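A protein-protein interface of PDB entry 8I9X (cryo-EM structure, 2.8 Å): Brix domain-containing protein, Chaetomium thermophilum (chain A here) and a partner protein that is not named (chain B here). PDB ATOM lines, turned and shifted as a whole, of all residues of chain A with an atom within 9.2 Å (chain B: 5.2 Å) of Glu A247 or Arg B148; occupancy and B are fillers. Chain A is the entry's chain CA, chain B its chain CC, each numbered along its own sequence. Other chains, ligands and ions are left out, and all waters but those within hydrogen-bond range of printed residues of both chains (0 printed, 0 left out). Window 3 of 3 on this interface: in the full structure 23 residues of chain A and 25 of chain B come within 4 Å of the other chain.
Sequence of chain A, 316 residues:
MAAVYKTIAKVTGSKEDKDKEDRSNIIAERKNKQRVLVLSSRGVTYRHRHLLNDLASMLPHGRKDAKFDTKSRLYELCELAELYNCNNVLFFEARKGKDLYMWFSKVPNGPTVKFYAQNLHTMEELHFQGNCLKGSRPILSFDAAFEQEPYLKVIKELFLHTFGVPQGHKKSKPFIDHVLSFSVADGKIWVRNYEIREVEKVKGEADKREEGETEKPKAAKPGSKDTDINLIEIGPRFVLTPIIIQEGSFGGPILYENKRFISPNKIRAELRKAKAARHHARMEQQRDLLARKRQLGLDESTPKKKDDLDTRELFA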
ATOM      1  N   SER A 105       3.439  30.209 -12.247  1.00  0.00           N
ATOM      2  CA  SER A 105       4.748  29.606 -12.599  1.00  0.00           C
ATOM      3  C   SER A 105       4.748  28.119 -12.297  1.00  0.00           C
ATOM      4  O   SER A 105       3.846  27.640 -11.614  1.00  0.00           O
ATOM      5  CB  SER A 105       5.889  30.258 -11.881  1.00  0.00           C
ATOM      6  OG  SER A 105       7.128  29.697 -12.270  1.00  0.00           O
ATOM      7  N   LYS A 106       5.820  27.478 -12.737  1.00  0.00           N
ATOM      8  CA  LYS A 106       6.110  26.073 -12.421  1.00  0.00           C
ATOM      9  C   LYS A 106       7.516  26.104 -11.824  1.00  0.00           C
ATOM     10  O   LYS A 106       8.434  26.522 -12.528  1.00  0.00           O
ATOM     11  CB  LYS A 106       6.044  25.203 -13.674  1.00  0.00           C
ATOM     12  CG  LYS A 106       4.647  24.851 -14.150  1.00  0.00           C
ATOM     13  CD  LYS A 106       4.079  23.635 -13.472  1.00  0.00           C
ATOM     14  CE  LYS A 106       5.083  22.526 -13.253  1.00  0.00           C
ATOM     15  NZ  LYS A 106       4.421  21.207 -13.150  1.00  0.00           N
ATOM     16  N   VAL A 107       7.673  25.701 -10.578  1.00  0.00           N
ATOM     17  CA  VAL A 107       8.953  25.747  -9.838  1.00  0.00           C
ATOM     18  C   VAL A 107       9.509  24.333  -9.829  1.00  0.00           C
ATOM     19  O   VAL A 107       8.729  23.411  -9.584  1.00  0.00           O
ATOM     20  CB  VAL A 107       8.730  26.355  -8.441  1.00  0.00           C
ATOM     21  CG1 VAL A 107       7.295  26.235  -7.962  1.00  0.00           C
ATOM     22  CG2 VAL A 107       9.699  25.831  -7.395  1.00  0.00           C
ATOM     23  N   PRO A 108      10.801  24.138 -10.157  1.00  0.00           N
ATOM     24  CA  PRO A 108      11.770  25.233 -10.201  1.00  0.00           C
ATOM     25  C   PRO A 108      12.331  25.743 -11.524  1.00  0.00           C
ATOM     26  O   PRO A 108      13.128  26.638 -11.469  1.00  0.00           O
ATOM     27  CB  PRO A 108      12.976  24.471  -9.664  1.00  0.00           C
ATOM     28  CG  PRO A 108      12.905  23.111 -10.294  1.00  0.00           C
ATOM     29  CD  PRO A 108      11.428  22.841 -10.443  1.00  0.00           C
ATOM     30  N   ASN A 109      11.903  25.186 -12.655  1.00  0.00           N
ATOM     31  CA  ASN A 109      12.569  25.499 -13.935  1.00  0.00           C
ATOM     32  C   ASN A 109      11.558  25.694 -15.045  1.00  0.00           C
ATOM     33  O   ASN A 109      11.982  25.733 -16.200  1.00  0.00           O
ATOM     34  CB  ASN A 109      13.527  24.361 -14.305  1.00  0.00           C
ATOM     35  CG  ASN A 109      13.060  22.994 -13.860  1.00  0.00           C
ATOM     36  OD1 ASN A 109      11.876  22.675 -13.934  1.00  0.00           O
ATOM     37  ND2 ASN A 109      13.990  22.173 -13.408  1.00  0.00           N
ATOM     38  N   GLY A 110      10.283  25.856 -14.721  1.00  0.00           N
ATOM     39  CA  GLY A 110       9.259  25.856 -15.784  1.00  0.00           C
ATOM     40  C   GLY A 110       9.042  27.200 -16.393  1.00  0.00           C
ATOM     41  O   GLY A 110       9.859  28.078 -16.140  1.00  0.00           O
ATOM     42  N   PRO A 111       7.996  27.404 -17.204  1.00  0.00           N
ATOM     43  CA  PRO A 111       7.675  28.743 -17.694  1.00  0.00           C
ATOM     44  C   PRO A 111       6.948  29.588 -16.633  1.00  0.00           C
ATOM     45  O   PRO A 111       6.381  29.016 -15.743  1.00  0.00           O
ATOM     46  CB  PRO A 111       6.765  28.448 -18.889  1.00  0.00           C
ATOM     47  CG  PRO A 111       6.861  26.954 -19.116  1.00  0.00           C
ATOM     48  CD  PRO A 111       7.133  26.371 -17.750  1.00  0.00           C
ATOM     49  N   THR A 112       7.001  30.912 -16.733  1.00  0.00           N
ATOM     50  CA  THR A 112       6.230  31.802 -15.833  1.00  0.00           C
ATOM     51  C   THR A 112       5.433  32.756 -16.712  1.00  0.00           C
ATOM     52  O   THR A 112       5.904  33.089 -17.796  1.00  0.00           O
ATOM     53  CB  THR A 112       7.123  32.573 -14.852  1.00  0.00           C
ATOM     54  OG1 THR A 112       6.442  32.685 -13.608  1.00  0.00           O
ATOM     55  CG2 THR A 112       7.455  33.976 -15.298  1.00  0.00           C
ATOM     56  N   VAL A 113       4.257  33.169 -16.265  1.00  0.00           N
ATOM     57  CA  VAL A 113       3.496  34.200 -17.017  1.00  0.00           C
ATOM     58  C   VAL A 113       3.053  35.313 -16.062  1.00  0.00           C
ATOM     59  O   VAL A 113       2.579  35.003 -14.978  1.00  0.00           O
ATOM     60  CB  VAL A 113       2.334  33.583 -17.819  1.00  0.00           C
ATOM     61  CG1 VAL A 113       1.356  32.787 -16.980  1.00  0.00           C
ATOM     62  CG2 VAL A 113       1.623  34.602 -18.692  1.00  0.00           C
ATOM     63  N   VAL A 154       1.088  27.969 -23.914  1.00  0.00           N
ATOM     64  CA  VAL A 154       1.910  27.866 -22.680  1.00  0.00           C
ATOM     65  C   VAL A 154       1.046  28.326 -21.509  1.00  0.00           C
ATOM     66  O   VAL A 154       1.100  27.672 -20.460  1.00  0.00           O
ATOM     67  CB  VAL A 154       3.224  28.655 -22.823  1.00  0.00           C
ATOM     68  CG1 VAL A 154       4.041  28.647 -21.542  1.00  0.00           C
ATOM     69  CG2 VAL A 154       4.050  28.138 -23.986  1.00  0.00           C
ATOM     70  N   ILE A 244       4.278  39.347 -19.994  1.00  0.00           N
ATOM     71  CA  ILE A 244       5.516  38.671 -20.366  1.00  0.00           C
ATOM     72  C   ILE A 244       5.375  37.178 -20.105  1.00  0.00           C
ATOM     73  O   ILE A 244       4.684  36.757 -19.175  1.00  0.00           O
ATOM     74  CB  ILE A 244       6.738  39.235 -19.607  1.00  0.00           C
ATOM     75  CG1 ILE A 244       6.520  39.152 -18.093  1.00  0.00           C
ATOM     76  CG2 ILE A 244       7.063  40.645 -20.064  1.00  0.00           C
ATOM     77  CD1 ILE A 244       7.782  39.313 -17.284  1.00  0.00           C
ATOM     78  N   ILE A 245       6.027  36.383 -20.949  1.00  0.00           N
ATOM     79  CA  ILE A 245       6.298  34.976 -20.683  1.00  0.00           C
ATOM     80  C   ILE A 245       7.809  34.826 -20.742  1.00  0.00           C
ATOM     81  O   ILE A 245       8.426  35.116 -21.775  1.00  0.00           O
ATOM     82  CB  ILE A 245       5.613  34.041 -21.687  1.00  0.00           C
ATOM     83  CG1 ILE A 245       4.097  34.207 -21.622  1.00  0.00           C
ATOM     84  CG2 ILE A 245       6.000  32.596 -21.419  1.00  0.00           C
ATOM     85  CD1 ILE A 245       3.355  33.289 -22.552  1.00  0.00           C
ATOM     86  N   GLN A 246       8.408  34.387 -19.645  1.00  0.00           N
ATOM     87  CA  GLN A 246       9.853  34.262 -19.559  1.00  0.00           C
ATOM     88  C   GLN A 246      10.246  32.828 -19.229  1.00  0.00           C
ATOM     89  O   GLN A 246       9.664  32.197 -18.341  1.00  0.00           O
ATOM     90  CB  GLN A 246      10.422  35.258 -18.538  1.00  0.00           C
ATOM     91  CG  GLN A 246       9.996  35.032 -17.114  1.00  0.00           C
ATOM     92  CD  GLN A 246      10.535  36.082 -16.163  1.00  0.00           C
ATOM     93  OE1 GLN A 246      11.284  36.972 -16.562  1.00  0.00           O
ATOM     94  NE2 GLN A 246      10.143  35.990 -14.899  1.00  0.00           N
ATOM     95  N   GLU A 247      11.223  32.318 -19.971  1.00  0.00           N
ATOM     96  CA  GLU A 247      11.693  30.943 -19.830  1.00  0.00           C
ATOM     97  C   GLU A 247      12.466  30.833 -18.525  1.00  0.00           C
ATOM     98  O   GLU A 247      13.643  31.191 -18.452  1.00  0.00           O
ATOM     99  CB  GLU A 247      12.560  30.551 -21.019  1.00  0.00           C
ATOM    100  CG  GLU A 247      13.107  29.143 -20.946  1.00  0.00           C
ATOM    101  CD  GLU A 247      14.355  28.962 -21.783  1.00  0.00           C
ATOM    102  OE1 GLU A 247      15.117  29.938 -21.941  1.00  0.00           O
ATOM    103  OE2 GLU A 247      14.567  27.843 -22.293  1.00  0.00           O
ATOM    104  N   GLY A 248      11.789  30.352 -17.493  1.00  0.00           N
ATOM    105  CA  GLY A 248      12.358  30.352 -16.139  1.00  0.00           C
ATOM    106  C   GLY A 248      11.277  30.461 -15.093  1.00  0.00           C
ATOM    107  O   GLY A 248      10.139  30.755 -15.472  1.00  0.00           O
ATOM    108  N   SER A 249      11.607  30.241 -13.825  1.00  0.00           N
ATOM    109  CA  SER A 249      10.568  30.126 -12.775  1.00  0.00           C
ATOM    110  C   SER A 249      10.074  31.500 -12.338  1.00  0.00           C
ATOM    111  O   SER A 249       8.853  31.677 -12.326  1.00  0.00           O
ATOM    112  CB  SER A 249      11.054  29.382 -11.611  1.00  0.00           C
ATOM    113  OG  SER A 249       9.965  28.877 -10.858  1.00  0.00           O
ATOM    114  N   PHE A 250      10.952  32.421 -11.977  1.00  0.00           N
ATOM    115  CA  PHE A 250      10.570  33.847 -12.066  1.00  0.00           C
ATOM    116  C   PHE A 250      11.772  34.616 -12.622  1.00  0.00           C
ATOM    117  O   PHE A 250      12.144  35.635 -12.041  1.00  0.00           O
ATOM    118  CB  PHE A 250      10.098  34.390 -10.711  1.00  0.00           C
ATOM    119  CG  PHE A 250       8.793  33.864 -10.178  1.00  0.00           C
ATOM    120  CD1 PHE A 250       7.601  34.488 -10.491  1.00  0.00           C
ATOM    121  CD2 PHE A 250       8.758  32.764  -9.339  1.00  0.00           C
ATOM    122  CE1 PHE A 250       6.398  34.011 -10.000  1.00  0.00           C
ATOM    123  CE2 PHE A 250       7.554  32.284  -8.851  1.00  0.00           C
ATOM    124  CZ  PHE A 250       6.378  32.909  -9.181  1.00  0.00           C
ATOM    125  N   GLY A 251      12.355  34.122 -13.713  1.00  0.00           N
ATOM    126  CA  GLY A 251      13.439  34.829 -14.413  1.00  0.00           C
ATOM    127  C   GLY A 251      13.786  34.176 -15.736  1.00  0.00           C
ATOM    128  O   GLY A 251      12.892  33.565 -16.336  1.00  0.00           O
ATOM    129  N   GLY A 252      15.035  34.295 -16.181  1.00  0.00           N
ATOM    130  CA  GLY A 252      15.452  33.762 -17.452  1.00  0.00           C
ATOM    131  C   GLY A 252      15.001  34.635 -18.601  1.00  0.00           C
ATOM    132  O   GLY A 252      14.349  35.665 -18.411  1.00  0.00           O
ATOM    133  N   PRO A 253      15.343  34.235 -19.822  1.00  0.00           N
ATOM    134  CA  PRO A 253      14.991  35.045 -20.989  1.00  0.00           C
ATOM    135  C   PRO A 253      13.487  35.123 -21.188  1.00  0.00           C
ATOM    136  O   PRO A 253      12.733  34.213 -20.839  1.00  0.00           O
ATOM    137  CB  PRO A 253      15.662  34.307 -22.153  1.00  0.00           C
ATOM    138  CG  PRO A 253      16.700  33.454 -21.514  1.00  0.00           C
ATOM    139  CD  PRO A 253      16.137  33.056 -20.196  1.00  0.00           C
ATOM    140  N   ILE A 254      13.061  36.238 -21.763  1.00  0.00           N
ATOM    141  CA  ILE A 254      11.657  36.474 -22.071  1.00  0.00           C
ATOM    142  C   ILE A 254      11.329  35.832 -23.411  1.00  0.00           C
ATOM    143  O   ILE A 254      12.016  36.071 -24.411  1.00  0.00           O
ATOM    144  CB  ILE A 254      11.345  37.979 -22.089  1.00  0.00           C
ATOM    145  CG1 ILE A 254      11.560  38.589 -20.705  1.00  0.00           C
ATOM    146  CG2 ILE A 254       9.936  38.228 -22.575  1.00  0.00           C
ATOM    147  CD1 ILE A 254      11.518  40.089 -20.710  1.00  0.00           C
ATOM    148  N   LEU A 255      10.281  35.012 -23.431  1.00  0.00           N
ATOM    149  CA  LEU A 255       9.800  34.387 -24.655  1.00  0.00           C
ATOM    150  C   LEU A 255       8.677  35.157 -25.327  1.00  0.00           C
ATOM    151  O   LEU A 255       8.430  34.954 -26.517  1.00  0.00           O
ATOM    152  CB  LEU A 255       9.316  32.962 -24.367  1.00  0.00           C
ATOM    153  CG  LEU A 255      10.327  32.043 -23.687  1.00  0.00           C
ATOM    154  CD1 LEU A 255       9.735  30.661 -23.485  1.00  0.00           C
ATOM    155  CD2 LEU A 255      11.599  31.971 -24.508  1.00  0.00           C
ATOM    156  N   TYR A 256       7.995  36.031 -24.592  1.00  0.00           N
ATOM    157  CA  TYR A 256       6.893  36.825 -25.115  1.00  0.00           C
ATOM    158  C   TYR A 256       6.770  38.104 -24.304  1.00  0.00           C
ATOM    159  O   TYR A 256       6.843  38.070 -23.077  1.00  0.00           O
ATOM    160  CB  TYR A 256       5.572  36.053 -25.062  1.00  0.00           C
ATOM    161  CG  TYR A 256       4.407  36.796 -25.664  1.00  0.00           C
ATOM    162  CD1 TYR A 256       4.297  36.971 -27.035  1.00  0.00           C
ATOM    163  CD2 TYR A 256       3.421  37.338 -24.854  1.00  0.00           C
ATOM    164  CE1 TYR A 256       3.231  37.655 -27.580  1.00  0.00           C
ATOM    165  CE2 TYR A 256       2.354  38.022 -25.389  1.00  0.00           C
ATOM    166  CZ  TYR A 256       2.262  38.177 -26.752  1.00  0.00           C
ATOM    167  OH  TYR A 256       1.198  38.863 -27.290  1.00  0.00           O
ATOM    168  N   ARG B 138      22.433  22.164 -12.802  1.00  0.00           N
ATOM    169  CA  ARG B 138      23.228  21.772 -13.955  1.00  0.00           C
ATOM    170  C   ARG B 138      22.989  22.762 -15.089  1.00  0.00           C
ATOM    171  O   ARG B 138      22.028  23.533 -15.077  1.00  0.00           O
ATOM    172  CB  ARG B 138      22.933  20.323 -14.371  1.00  0.00           C
ATOM    173  CG  ARG B 138      21.616  20.083 -15.066  1.00  0.00           C
ATOM    174  CD  ARG B 138      21.411  18.577 -15.244  1.00  0.00           C
ATOM    175  NE  ARG B 138      20.160  18.205 -15.898  1.00  0.00           N
ATOM    176  CZ  ARG B 138      19.749  18.648 -17.080  1.00  0.00           C
ATOM    177  NH1 ARG B 138      20.504  19.433 -17.831  1.00  0.00           N
ATOM    178  NH2 ARG B 138      18.558  18.267 -17.535  1.00  0.00           N
ATOM    179  N   ILE B 139      23.897  22.751 -16.063  1.00  0.00           N
ATOM    180  CA  ILE B 139      24.020  23.822 -17.046  1.00  0.00           C
ATOM    181  C   ILE B 139      23.408  23.381 -18.368  1.00  0.00           C
ATOM    182  O   ILE B 139      23.692  22.281 -18.857  1.00  0.00           O
ATOM    183  CB  ILE B 139      25.491  24.223 -17.243  1.00  0.00           C
ATOM    184  CG1 ILE B 139      26.141  24.560 -15.904  1.00  0.00           C
ATOM    185  CG2 ILE B 139      25.594  25.411 -18.180  1.00  0.00           C
ATOM    186  CD1 ILE B 139      25.508  25.714 -15.200  1.00  0.00           C
ATOM    187  N   GLU B 140      22.569  24.237 -18.946  1.00  0.00           N
ATOM    188  CA  GLU B 140      22.105  24.092 -20.320  1.00  0.00           C
ATOM    189  C   GLU B 140      22.149  25.465 -20.980  1.00  0.00           C
ATOM    190  O   GLU B 140      22.679  26.430 -20.423  1.00  0.00           O
ATOM    191  CB  GLU B 140      20.695  23.492 -20.398  1.00  0.00           C
ATOM    192  CG  GLU B 140      20.401  22.367 -19.436  1.00  0.00           C
ATOM    193  CD  GLU B 140      19.274  21.482 -19.932  1.00  0.00           C
ATOM    194  OE1 GLU B 140      18.548  21.909 -20.855  1.00  0.00           O
ATOM    195  OE2 GLU B 140      19.113  20.362 -19.409  1.00  0.00           O
ATOM    196  N   LYS B 141      21.557  25.559 -22.164  1.00  0.00           N
ATOM    197  CA  LYS B 141      21.489  26.802 -22.911  1.00  0.00           C
ATOM    198  C   LYS B 141      20.106  27.430 -22.779  1.00  0.00           C
ATOM    199  O   LYS B 141      19.086  26.740 -22.716  1.00  0.00           O
ATOM    200  CB  LYS B 141      21.817  26.570 -24.389  1.00  0.00           C
ATOM    201  CG  LYS B 141      23.216  26.031 -24.634  1.00  0.00           C
ATOM    202  CD  LYS B 141      24.274  27.008 -24.153  1.00  0.00           C
ATOM    203  CE  LYS B 141      24.269  28.275 -24.990  1.00  0.00           C
ATOM    204  NZ  LYS B 141      24.654  28.001 -26.402  1.00  0.00           N
ATOM    205  N   ASP B 142      20.088  28.760 -22.740  1.00  0.00           N
ATOM    206  CA  ASP B 142      18.860  29.537 -22.750  1.00  0.00           C
ATOM    207  C   ASP B 142      18.221  29.491 -24.133  1.00  0.00           C
ATOM    208  O   ASP B 142      18.755  28.912 -25.081  1.00  0.00           O
ATOM    209  CB  ASP B 142      19.130  30.989 -22.343  1.00  0.00           C
ATOM    210  CG  ASP B 142      19.480  31.137 -20.879  1.00  0.00           C
ATOM    211  OD1 ASP B 142      18.997  30.327 -20.067  1.00  0.00           O
ATOM    212  OD2 ASP B 142      20.230  32.075 -20.538  1.00  0.00           O
ATOM    213  N   ALA B 143      17.052  30.119 -24.245  1.00  0.00           N
ATOM    214  CA  ALA B 143      16.438  30.325 -25.548  1.00  0.00           C
ATOM    215  C   ALA B 143      17.163  31.382 -26.366  1.00  0.00           C
ATOM    216  O   ALA B 143      17.026  31.401 -27.594  1.00  0.00           O
ATOM    217  CB  ALA B 143      14.968  30.715 -25.382  1.00  0.00           C
ATOM    218  N   GLY B 146      22.087  31.705 -23.860  1.00  0.00           N
ATOM    219  CA  GLY B 146      22.717  32.007 -22.600  1.00  0.00           C
ATOM    220  C   GLY B 146      22.855  30.781 -21.717  1.00  0.00           C
ATOM    221  O   GLY B 146      22.639  29.644 -22.137  1.00  0.00           O
ATOM    222  N   ILE B 147      23.231  31.035 -20.468  1.00  0.00           N
ATOM    223  CA  ILE B 147      23.380  29.990 -19.462  1.00  0.00           C
ATOM    224  C   ILE B 147      22.031  29.762 -18.798  1.00  0.00           C
ATOM    225  O   ILE B 147      21.380  30.717 -18.357  1.00  0.00           O
ATOM    226  CB  ILE B 147      24.449  30.367 -18.422  1.00  0.00           C
ATOM    227  CG1 ILE B 147      25.819  30.497 -19.089  1.00  0.00           C
ATOM    228  CG2 ILE B 147      24.496  29.340 -17.305  1.00  0.00           C
ATOM    229  CD1 ILE B 147      26.874  31.112 -18.199  1.00  0.00           C
ATOM    230  N   ARG B 148      21.605  28.503 -18.726  1.00  0.00           N
ATOM    231  CA  ARG B 148      20.361  28.130 -18.071  1.00  0.00           C
ATOM    232  C   ARG B 148      20.672  27.170 -16.934  1.00  0.00           C
ATOM    233  O   ARG B 148      21.350  26.159 -17.137  1.00  0.00           O
ATOM    234  CB  ARG B 148      19.387  27.485 -19.059  1.00  0.00           C
ATOM    235  CG  ARG B 148      18.029  27.157 -18.470  1.00  0.00           C
ATOM    236  CD  ARG B 148      17.236  26.249 -19.390  1.00  0.00           C
ATOM    237  NE  ARG B 148      16.222  25.489 -18.670  1.00  0.00           N
ATOM    238  CZ  ARG B 148      15.048  25.977 -18.295  1.00  0.00           C
ATOM    239  NH1 ARG B 148      14.702  27.226 -18.555  1.00  0.00           N
ATOM    240  NH2 ARG B 148      14.199  25.190 -17.639  1.00  0.00           N
ATOM    241  N   TYR B 149      20.173  27.489 -15.746  1.00  0.00           N
ATOM    242  CA  TYR B 149      20.393  26.682 -14.554  1.00  0.00           C
ATOM    243  C   TYR B 149      19.173  25.789 -14.356  1.00  0.00           C
ATOM    244  O   TYR B 149      18.091  26.275 -14.013  1.00  0.00           O
ATOM    245  CB  TYR B 149      20.622  27.577 -13.340  1.00  0.00           C
ATOM    246  CG  TYR B 149      21.886  28.400 -13.418  1.00  0.00           C
ATOM    247  CD1 TYR B 149      23.108  27.809 -13.691  1.00  0.00           C
ATOM    248  CD2 TYR B 149      21.849  29.775 -13.244  1.00  0.00           C
ATOM    249  CE1 TYR B 149      24.263  28.563 -13.770  1.00  0.00           C
ATOM    250  CE2 TYR B 149      22.997  30.535 -13.327  1.00  0.00           C
ATOM    251  CZ  TYR B 149      24.202  29.923 -13.588  1.00  0.00           C
ATOM    252  OH  TYR B 149      25.352  30.672 -13.669  1.00  0.00           O
ATOM    253  N   VAL B 150      19.318  24.517 -14.690  1.00  0.00           N
ATOM    254  CA  VAL B 150      18.220  23.546 -14.463  1.00  0.00           C
ATOM    255  C   VAL B 150      18.408  22.951 -13.078  1.00  0.00           C
ATOM    256  O   VAL B 150      19.418  22.280 -12.856  1.00  0.00           O
ATOM    257  CB  VAL B 150      18.195  22.471 -15.556  1.00  0.00           C
ATOM    258  CG1 VAL B 150      17.251  21.333 -15.208  1.00  0.00           C
ATOM    259  CG2 VAL B 150      17.839  23.062 -16.906  1.00  0.00           C
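Among the printed residues, merely in contact across the chains: Pro A253 with Asp B142 (3.6 Å), Leu A255 with Ala B143 (3.7 Å), Asn A109 with Val B150 (3.8 Å) and Glu A247 with Asp B142 (3.8 Å).
Printed residues of chain B that touch a printed residue of chain A: Asp B142, Ala B143, Arg B148 and Val B150. Hydrophobic or aromatic side chains of chain B within 4 Å of the printed part of chain A: Ala B143 and Val B150. Among the printed residues, 7 pairs touch across the chains. Among the printed residues, Asp or Glu carboxylates within 4 Å of a Lys or Arg side-chain nitrogen of the other chain: Glu A247 with Arg B148.
The side-chain carboxylate (OE2) of Glu A247 lies within salt-bridge range of the guanidinium group (NH1) of Arg B148. The side-chain carboxylate of Glu A247 is in hydrogen-bond range of the backbone NH of Ala B143. O of Asn A109 lies within hydrogen-bond range of NH2 of Arg B148.
Of chain B, only Asp B142 (3.8 Å), Ala B143 (3.0 Å) and Arg B148 (3.5 Å) come within 4 Å of Glu A247. Of chain A, only Asn A109 and Glu A247 come within 4 Å of Arg B148. Asp B142 touches just these residues of chain A: Glu A247 and Pro A253. Of the printed residues of chain B, Leu A255 touches Ala B143 (3.7 Å). Printed residues of chain B within 4 Å of Asn A109: Arg B148 (2.7 Å) and Val B150 (3.8 Å). Gly A252 touches none of the printed residues of chain B. The nearest residue of chain B that does not touch Glu A247 is Lys B141 (4.7 Å). The nearest residue of chain A that does not touch Arg B148 is Gly A248 (4.4 Å). The nearest printed residue of chain A that does not touch Val B150 is Pro A108 (6.2 Å).
The side-chain carboxylate of Asp B142 lies within hydrogen-bond range of the backbone NH of Ile B147. The side-chain carboxylate of Asp B142 lies close to the backbone NH of Arg B148, at 3.5 Å. O of Glu B140 lies within hydrogen-bond range of N of Arg B148 (2.9 Å). The backbone NH (N) of Glu A247 sits at hydrogen-bond distance from the backbone carbonyl oxygen (O) of Pro A253, 2.6 Å away. The backbone carbonyl oxygen (O) of Arg B138 is in hydrogen-bond range of the backbone NH (N) of Val B150 (2.9 Å). The backbone NH of Leu A255 is in hydrogen-bond range of the backbone carbonyl oxygen of Ile A245, 2.5 Å away.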
